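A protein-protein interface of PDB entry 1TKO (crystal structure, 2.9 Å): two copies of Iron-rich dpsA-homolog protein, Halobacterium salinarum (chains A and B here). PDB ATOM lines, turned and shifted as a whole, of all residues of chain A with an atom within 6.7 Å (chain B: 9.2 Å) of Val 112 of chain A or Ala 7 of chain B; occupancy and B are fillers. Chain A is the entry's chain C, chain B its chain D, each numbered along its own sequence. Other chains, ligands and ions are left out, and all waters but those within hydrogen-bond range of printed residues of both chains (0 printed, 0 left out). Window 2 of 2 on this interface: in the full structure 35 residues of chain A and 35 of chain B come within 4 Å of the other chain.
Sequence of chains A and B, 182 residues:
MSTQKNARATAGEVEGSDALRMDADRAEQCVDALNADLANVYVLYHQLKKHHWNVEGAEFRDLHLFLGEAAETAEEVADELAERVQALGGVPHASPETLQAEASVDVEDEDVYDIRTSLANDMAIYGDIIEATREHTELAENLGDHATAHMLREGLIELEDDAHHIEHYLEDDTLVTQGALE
The backbone carbonyl oxygen (O) of Asp 109 of chain A sits at hydrogen-bond distance from the side-chain amino group (NZ) of Lys 50 of chain A (3.0 Å).
The side-chain carboxylate (OD2) of Asp 109 of chain A sits at hydrogen-bond distance from the side-chain hydroxyl (OH) of Tyr 113 of chain A (2.6 Å).
The backbone carbonyl oxygen of Asp 114 of chain A lies within hydrogen-bond range of the side-chain hydroxyl of Ser 118 of chain A (2.9 Å).
The side-chain carboxylate (OE2) of Glu 13 of chain B lies close to the backbone NH (N) of Thr 10 of chain B (3.2 Å).
The backbone carbonyl oxygen (O) of Lys 50 of chain A sits at hydrogen-bond distance from the side-chain amide nitrogen (ND2) of Asn 54 of chain A, 3.1 Å away.
OE2 of Glu 108 of chain A lies within salt-bridge range of NZ of Lys 50 of chain A, 3.0 Å away.
Printed residues of chain B within 4 Å of Val 112 of chain A: Ala 7 (3.3 Å), Arg 8 (2.4 Å), Ala 9 (2.9 Å) and Val 91 (3.9 Å).
Of the printed residues of chain A, Ala 7 of chain B touches Val 112 and Tyr 113.
Of the printed residues of chain B, Asp 111 of chain A touches Ala 9, Thr 10 and Ala 11.
Tyr 113 of chain A touches just one residue of chain B: Ala 7.
Of the printed residues of chain A, Pro 92 of chain B touches Asn 54.
Of the printed residues of chain B, Asn 54 of chain A touches Gln 86 and Pro 92.
Printed residues of chain A within 4 Å of His 93 of chain B: Glu 110 (3.7 Å).
Of the printed residues of chain B, Asp 114 of chain A touches Arg 8.
Glu 108 of chain A touches none of the printed residues of chain B.
The nearest residue of chain A that does not touch Ala 7 of chain B is Asp 111 of chain A (4.2 Å).
The nearest printed residue of chain A that does not touch Ala 94 of chain B is Asn 54 of chain A (6.1 Å).
No position is printed for both chains.
Of the 16 pairs that touch across the chains among the printed residues, none has its exchanged pair printed and touching as well.
Lys 50 of chain A touches Ala 94 of chain B (CD to CB, 3.5 Å).
OD1 of Asn 54 of chain A touches CG of Gln 86 of chain B (3.3 Å).
Pro 92 of chain B touches Asn 54 of chain A (CD to OD1, 3.98 Å).
O of Glu 110 of chain A touches CB of Ala 11 of chain B, at 3.1 Å.
Glu 110 of chain A touches Val 91 of chain B.
Glu 110 of chain A touches His 93 of chain B.
Val 112 of chain A touches Ala 7 of chain B (O to C, 3.3 Å).
Val 91 of chain B touches Val 112 of chain A.
Tyr 113 of chain A touches Ala 7 of chain B.
Arg 8 of chain B touches Asp 114 of chain A (CD to CA, 3.6 Å).
Of the 11 printed residues of chain A, 7 touch a printed residue of chain B.
Printed residues of chain B that touch a printed residue of chain A: Ala 7, Arg 8, Ala 9, Thr 10, Ala 11, Gln 86, Val 91, Pro 92, His 93 and Ala 94.
Hydrophobic or aromatic side chains of chain B that line the printed part of chain A: Ala 7, Ala 9, Ala 11, Val 91, Pro 92 and Ala 94.
Among the printed residues, 16 pairs touch across the chains.
Among the printed residues, no Asp or Glu carboxylate lies within 4 Å of a Lys or Arg side-chain nitrogen of the other chain.
The backbone NH (N) of Val 112 of chain A is in hydrogen-bond range of the backbone carbonyl oxygen (O) of Ala 9 of chain B, at 2.9 Å.
The backbone NH (N) of Ala 11 of chain B sits at hydrogen-bond distance from the side-chain carboxylate (OD1) of Asp 111 of chain A, 3.0 Å away.
The side-chain hydroxyl (OG1) of Thr 10 of chain B sits close to the side-chain carboxylate (OD1) of Asp 111 of chain A, at 3.4 Å.
The backbone carbonyl oxygen (O) of Ala 9 of chain B sits close to the side-chain carboxylate (OD1) of Asp 111 of chain A (3.5 Å).
The backbone carbonyl oxygen (O) of Val 112 of chain A sits at hydrogen-bond distance from the backbone NH (N) of Arg 8 of chain B (2.4 Å).
The side-chain carboxylate (OE2) of Glu 110 of chain A is in hydrogen-bond range of the backbone NH (N) of Ala 94 of chain B (2.9 Å).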
ATOM      1  N   LYS A  50       2.859 -27.810  14.676  1.00  0.00           N
ATOM      2  CA  LYS A  50       3.288 -26.843  15.663  1.00  0.00           C
ATOM      3  C   LYS A  50       2.265 -26.725  16.784  1.00  0.00           C
ATOM      4  O   LYS A  50       2.609 -26.891  17.952  1.00  0.00           O
ATOM      5  CB  LYS A  50       3.497 -25.487  14.997  1.00  0.00           C
ATOM      6  CG  LYS A  50       3.790 -24.362  15.955  1.00  0.00           C
ATOM      7  CD  LYS A  50       3.990 -23.075  15.196  1.00  0.00           C
ATOM      8  CE  LYS A  50       4.164 -21.877  16.124  1.00  0.00           C
ATOM      9  NZ  LYS A  50       4.329 -20.615  15.349  1.00  0.00           N
ATOM     10  N   ASN A  54       2.579 -27.741  20.809  1.00  0.00           N
ATOM     11  CA  ASN A  54       2.478 -26.724  21.845  1.00  0.00           C
ATOM     12  C   ASN A  54       1.208 -26.575  22.672  1.00  0.00           C
ATOM     13  O   ASN A  54       1.288 -26.164  23.818  1.00  0.00           O
ATOM     14  CB  ASN A  54       2.845 -25.359  21.240  1.00  0.00           C
ATOM     15  CG  ASN A  54       4.275 -25.311  20.729  1.00  0.00           C
ATOM     16  OD1 ASN A  54       5.231 -25.582  21.463  1.00  0.00           O
ATOM     17  ND2 ASN A  54       4.429 -24.963  19.470  1.00  0.00           N
ATOM     18  N   VAL A  55       0.045 -26.891  22.120  1.00  0.00           N
ATOM     19  CA  VAL A  55      -1.194 -26.727  22.872  1.00  0.00           C
ATOM     20  C   VAL A  55      -1.119 -27.174  24.342  1.00  0.00           C
ATOM     21  O   VAL A  55      -0.599 -28.242  24.663  1.00  0.00           O
ATOM     22  CB  VAL A  55      -2.370 -27.444  22.165  1.00  0.00           C
ATOM     23  CG1 VAL A  55      -2.188 -28.932  22.212  1.00  0.00           C
ATOM     24  CG2 VAL A  55      -3.670 -27.048  22.809  1.00  0.00           C
ATOM     25  N   GLU A 108       2.618 -18.399  10.809  1.00  0.00           N
ATOM     26  CA  GLU A 108       3.032 -17.731  12.046  1.00  0.00           C
ATOM     27  C   GLU A 108       4.541 -17.691  12.219  1.00  0.00           C
ATOM     28  O   GLU A 108       5.245 -18.627  11.834  1.00  0.00           O
ATOM     29  CB  GLU A 108       2.477 -18.457  13.276  1.00  0.00           C
ATOM     30  CG  GLU A 108       0.983 -18.586  13.367  1.00  0.00           C
ATOM     31  CD  GLU A 108       0.557 -19.327  14.623  1.00  0.00           C
ATOM     32  OE1 GLU A 108      -0.660 -19.364  14.884  1.00  0.00           O
ATOM     33  OE2 GLU A 108       1.424 -19.875  15.350  1.00  0.00           O
ATOM     34  N   ASP A 109       5.036 -16.614  12.824  1.00  0.00           N
ATOM     35  CA  ASP A 109       6.463 -16.511  13.090  1.00  0.00           C
ATOM     36  C   ASP A 109       6.735 -17.556  14.169  1.00  0.00           C
ATOM     37  O   ASP A 109       5.804 -18.033  14.819  1.00  0.00           O
ATOM     38  CB  ASP A 109       6.828 -15.118  13.592  1.00  0.00           C
ATOM     39  CG  ASP A 109       6.023 -14.706  14.803  1.00  0.00           C
ATOM     40  OD1 ASP A 109       6.314 -13.637  15.381  1.00  0.00           O
ATOM     41  OD2 ASP A 109       5.091 -15.442  15.181  1.00  0.00           O
ATOM     42  N   GLU A 110       7.997 -17.910  14.367  1.00  0.00           N
ATOM     43  CA  GLU A 110       8.348 -18.925  15.344  1.00  0.00           C
ATOM     44  C   GLU A 110       7.968 -18.713  16.810  1.00  0.00           C
ATOM     45  O   GLU A 110       8.480 -19.414  17.678  1.00  0.00           O
ATOM     46  CB  GLU A 110       9.834 -19.231  15.241  1.00  0.00           C
ATOM     47  CG  GLU A 110      10.224 -19.820  13.906  1.00  0.00           C
ATOM     48  CD  GLU A 110       9.429 -21.057  13.571  1.00  0.00           C
ATOM     49  OE1 GLU A 110       8.715 -21.033  12.542  1.00  0.00           O
ATOM     50  OE2 GLU A 110       9.517 -22.050  14.336  1.00  0.00           O
ATOM     51  N   ASP A 111       7.086 -17.767  17.113  1.00  0.00           N
ATOM     52  CA  ASP A 111       6.690 -17.605  18.507  1.00  0.00           C
ATOM     53  C   ASP A 111       5.467 -18.477  18.789  1.00  0.00           C
ATOM     54  O   ASP A 111       4.806 -18.935  17.861  1.00  0.00           O
ATOM     55  CB  ASP A 111       6.396 -16.139  18.840  1.00  0.00           C
ATOM     56  CG  ASP A 111       7.665 -15.351  19.202  1.00  0.00           C
ATOM     57  OD1 ASP A 111       8.586 -15.935  19.827  1.00  0.00           O
ATOM     58  OD2 ASP A 111       7.738 -14.144  18.880  1.00  0.00           O
ATOM     59  N   VAL A 112       5.172 -18.716  20.063  1.00  0.00           N
ATOM     60  CA  VAL A 112       4.031 -19.552  20.444  1.00  0.00           C
ATOM     61  C   VAL A 112       2.863 -18.743  21.020  1.00  0.00           C
ATOM     62  O   VAL A 112       3.018 -18.083  22.044  1.00  0.00           O
ATOM     63  CB  VAL A 112       4.452 -20.595  21.496  1.00  0.00           C
ATOM     64  CG1 VAL A 112       3.250 -21.424  21.927  1.00  0.00           C
ATOM     65  CG2 VAL A 112       5.550 -21.485  20.935  1.00  0.00           C
ATOM     66  N   TYR A 113       1.694 -18.807  20.384  1.00  0.00           N
ATOM     67  CA  TYR A 113       0.536 -18.067  20.873  1.00  0.00           C
ATOM     68  C   TYR A 113      -0.506 -18.939  21.564  1.00  0.00           C
ATOM     69  O   TYR A 113      -0.488 -20.156  21.427  1.00  0.00           O
ATOM     70  CB  TYR A 113      -0.125 -17.316  19.725  1.00  0.00           C
ATOM     71  CG  TYR A 113       0.848 -16.465  18.964  1.00  0.00           C
ATOM     72  CD1 TYR A 113       1.407 -16.913  17.773  1.00  0.00           C
ATOM     73  CD2 TYR A 113       1.261 -15.233  19.466  1.00  0.00           C
ATOM     74  CE1 TYR A 113       2.362 -16.153  17.098  1.00  0.00           C
ATOM     75  CE2 TYR A 113       2.213 -14.464  18.800  1.00  0.00           C
ATOM     76  CZ  TYR A 113       2.760 -14.928  17.618  1.00  0.00           C
ATOM     77  OH  TYR A 113       3.702 -14.165  16.960  1.00  0.00           O
ATOM     78  N   ASP A 114      -1.406 -18.308  22.313  1.00  0.00           N
ATOM     79  CA  ASP A 114      -2.462 -19.025  23.015  1.00  0.00           C
ATOM     80  C   ASP A 114      -3.209 -19.869  21.996  1.00  0.00           C
ATOM     81  O   ASP A 114      -3.115 -19.631  20.790  1.00  0.00           O
ATOM     82  CB  ASP A 114      -3.430 -18.051  23.682  1.00  0.00           C
ATOM     83  CG  ASP A 114      -3.914 -16.970  22.730  1.00  0.00           C
ATOM     84  OD1 ASP A 114      -3.101 -16.078  22.378  1.00  0.00           O
ATOM     85  OD2 ASP A 114      -5.099 -17.009  22.323  1.00  0.00           O
ATOM     86  N   SER A 118      -3.957 -19.294  17.770  1.00  0.00           N
ATOM     87  CA  SER A 118      -3.449 -20.317  16.858  1.00  0.00           C
ATOM     88  C   SER A 118      -4.589 -20.946  16.053  1.00  0.00           C
ATOM     89  O   SER A 118      -4.569 -20.938  14.825  1.00  0.00           O
ATOM     90  CB  SER A 118      -2.726 -21.408  17.644  1.00  0.00           C
ATOM     91  OG  SER A 118      -1.742 -20.858  18.490  1.00  0.00           O
ATOM     92  N   ALA B   7       2.201 -13.433  23.049  1.00  0.00           N
ATOM     93  CA  ALA B   7       2.763 -14.799  22.791  1.00  0.00           C
ATOM     94  C   ALA B   7       2.995 -15.546  24.101  1.00  0.00           C
ATOM     95  O   ALA B   7       3.412 -14.950  25.097  1.00  0.00           O
ATOM     96  CB  ALA B   7       4.081 -14.696  22.010  1.00  0.00           C
ATOM     97  N   ARG B   8       2.722 -16.849  24.101  1.00  0.00           N
ATOM     98  CA  ARG B   8       2.907 -17.665  25.297  1.00  0.00           C
ATOM     99  C   ARG B   8       4.366 -18.045  25.501  1.00  0.00           C
ATOM    100  O   ARG B   8       4.798 -18.271  26.627  1.00  0.00           O
ATOM    101  CB  ARG B   8       2.056 -18.936  25.225  1.00  0.00           C
ATOM    102  CG  ARG B   8       0.596 -18.738  25.555  1.00  0.00           C
ATOM    103  CD  ARG B   8      -0.129 -20.076  25.541  1.00  0.00           C
ATOM    104  NE  ARG B   8       0.224 -20.940  26.665  1.00  0.00           N
ATOM    105  CZ  ARG B   8      -0.138 -20.705  27.920  1.00  0.00           C
ATOM    106  NH1 ARG B   8      -0.860 -19.631  28.211  1.00  0.00           N
ATOM    107  NH2 ARG B   8       0.210 -21.550  28.882  1.00  0.00           N
ATOM    108  N   ALA B   9       5.117 -18.124  24.410  1.00  0.00           N
ATOM    109  CA  ALA B   9       6.529 -18.475  24.485  1.00  0.00           C
ATOM    110  C   ALA B   9       7.274 -17.843  23.318  1.00  0.00           C
ATOM    111  O   ALA B   9       6.678 -17.527  22.279  1.00  0.00           O
ATOM    112  CB  ALA B   9       6.709 -19.998  24.464  1.00  0.00           C
ATOM    113  N   THR B  10       8.576 -17.650  23.492  1.00  0.00           N
ATOM    114  CA  THR B  10       9.380 -17.059  22.447  1.00  0.00           C
ATOM    115  C   THR B  10      10.412 -18.034  21.920  1.00  0.00           C
ATOM    116  O   THR B  10      11.129 -18.674  22.685  1.00  0.00           O
ATOM    117  CB  THR B  10      10.087 -15.786  22.949  1.00  0.00           C
ATOM    118  OG1 THR B  10       9.146 -14.701  22.998  1.00  0.00           O
ATOM    119  CG2 THR B  10      11.252 -15.419  22.032  1.00  0.00           C
ATOM    120  N   ALA B  11      10.473 -18.149  20.600  1.00  0.00           N
ATOM    121  CA  ALA B  11      11.428 -19.044  19.974  1.00  0.00           C
ATOM    122  C   ALA B  11      12.791 -18.762  20.586  1.00  0.00           C
ATOM    123  O   ALA B  11      13.211 -17.613  20.670  1.00  0.00           O
ATOM    124  CB  ALA B  11      11.463 -18.805  18.468  1.00  0.00           C
ATOM    125  N   GLY B  12      13.473 -19.811  21.028  1.00  0.00           N
ATOM    126  CA  GLY B  12      14.782 -19.629  21.625  1.00  0.00           C
ATOM    127  C   GLY B  12      14.791 -19.803  23.131  1.00  0.00           C
ATOM    128  O   GLY B  12      15.813 -20.169  23.709  1.00  0.00           O
ATOM    129  N   GLU B  13      13.659 -19.549  23.775  1.00  0.00           N
ATOM    130  CA  GLU B  13      13.582 -19.670  25.223  1.00  0.00           C
ATOM    131  C   GLU B  13      13.364 -21.107  25.681  1.00  0.00           C
ATOM    132  O   GLU B  13      12.682 -21.882  25.021  1.00  0.00           O
ATOM    133  CB  GLU B  13      12.489 -18.743  25.747  1.00  0.00           C
ATOM    134  CG  GLU B  13      12.881 -17.259  25.635  1.00  0.00           C
ATOM    135  CD  GLU B  13      11.694 -16.296  25.693  1.00  0.00           C
ATOM    136  OE1 GLU B  13      11.937 -15.064  25.616  1.00  0.00           O
ATOM    137  OE2 GLU B  13      10.529 -16.770  25.804  1.00  0.00           O
ATOM    138  N   GLN B  86       9.601 -29.534  23.415  1.00  0.00           N
ATOM    139  CA  GLN B  86       8.492 -28.848  24.081  1.00  0.00           C
ATOM    140  C   GLN B  86       8.340 -29.336  25.517  1.00  0.00           C
ATOM    141  O   GLN B  86       7.922 -28.582  26.400  1.00  0.00           O
ATOM    142  CB  GLN B  86       7.194 -29.078  23.306  1.00  0.00           C
ATOM    143  CG  GLN B  86       6.173 -27.975  23.461  1.00  0.00           C
ATOM    144  CD  GLN B  86       5.405 -28.075  24.756  1.00  0.00           C
ATOM    145  OE1 GLN B  86       4.682 -27.142  25.152  1.00  0.00           O
ATOM    146  NE2 GLN B  86       5.539 -29.218  25.425  1.00  0.00           N
ATOM    147  N   GLY B  89      10.662 -27.660  28.016  1.00  0.00           N
ATOM    148  CA  GLY B  89      10.471 -26.225  28.113  1.00  0.00           C
ATOM    149  C   GLY B  89      10.876 -25.392  26.914  1.00  0.00           C
ATOM    150  O   GLY B  89      10.746 -24.167  26.952  1.00  0.00           O
ATOM    151  N   GLY B  90      11.347 -26.041  25.852  1.00  0.00           N
ATOM    152  CA  GLY B  90      11.771 -25.315  24.665  1.00  0.00           C
ATOM    153  C   GLY B  90      10.670 -25.027  23.664  1.00  0.00           C
ATOM    154  O   GLY B  90       9.499 -25.244  23.937  1.00  0.00           O
ATOM    155  N   VAL B  91      11.058 -24.515  22.503  1.00  0.00           N
ATOM    156  CA  VAL B  91      10.131 -24.195  21.429  1.00  0.00           C
ATOM    157  C   VAL B  91      10.688 -24.807  20.148  1.00  0.00           C
ATOM    158  O   VAL B  91      11.632 -24.289  19.554  1.00  0.00           O
ATOM    159  CB  VAL B  91       9.982 -22.662  21.242  1.00  0.00           C
ATOM    160  CG1 VAL B  91       9.255 -22.351  19.941  1.00  0.00           C
ATOM    161  CG2 VAL B  91       9.206 -22.078  22.398  1.00  0.00           C
ATOM    162  N   PRO B  92      10.106 -25.927  19.707  1.00  0.00           N
ATOM    163  CA  PRO B  92      10.542 -26.622  18.491  1.00  0.00           C
ATOM    164  C   PRO B  92      10.354 -25.810  17.215  1.00  0.00           C
ATOM    165  O   PRO B  92       9.373 -25.076  17.082  1.00  0.00           O
ATOM    166  CB  PRO B  92       9.689 -27.886  18.502  1.00  0.00           C
ATOM    167  CG  PRO B  92       8.403 -27.391  19.120  1.00  0.00           C
ATOM    168  CD  PRO B  92       8.901 -26.562  20.275  1.00  0.00           C
ATOM    169  N   HIS B  93      11.298 -25.942  16.284  1.00  0.00           N
ATOM    170  CA  HIS B  93      11.216 -25.229  15.015  1.00  0.00           C
ATOM    171  C   HIS B  93       9.916 -25.708  14.367  1.00  0.00           C
ATOM    172  O   HIS B  93       9.547 -26.875  14.515  1.00  0.00           O
ATOM    173  CB  HIS B  93      12.423 -25.570  14.124  1.00  0.00           C
ATOM    174  CG  HIS B  93      13.746 -25.143  14.696  1.00  0.00           C
ATOM    175  ND1 HIS B  93      13.953 -23.898  15.257  1.00  0.00           N
ATOM    176  CD2 HIS B  93      14.936 -25.793  14.780  1.00  0.00           C
ATOM    177  CE1 HIS B  93      15.208 -23.805  15.665  1.00  0.00           C
ATOM    178  NE2 HIS B  93      15.826 -24.939  15.387  1.00  0.00           N
ATOM    179  N   ALA B  94       9.212 -24.831  13.657  1.00  0.00           N
ATOM    180  CA  ALA B  94       7.952 -25.250  13.055  1.00  0.00           C
ATOM    181  C   ALA B  94       7.741 -24.976  11.569  1.00  0.00           C
ATOM    182  O   ALA B  94       7.426 -25.900  10.824  1.00  0.00           O
ATOM    183  CB  ALA B  94       6.798 -24.667  13.847  1.00  0.00           C
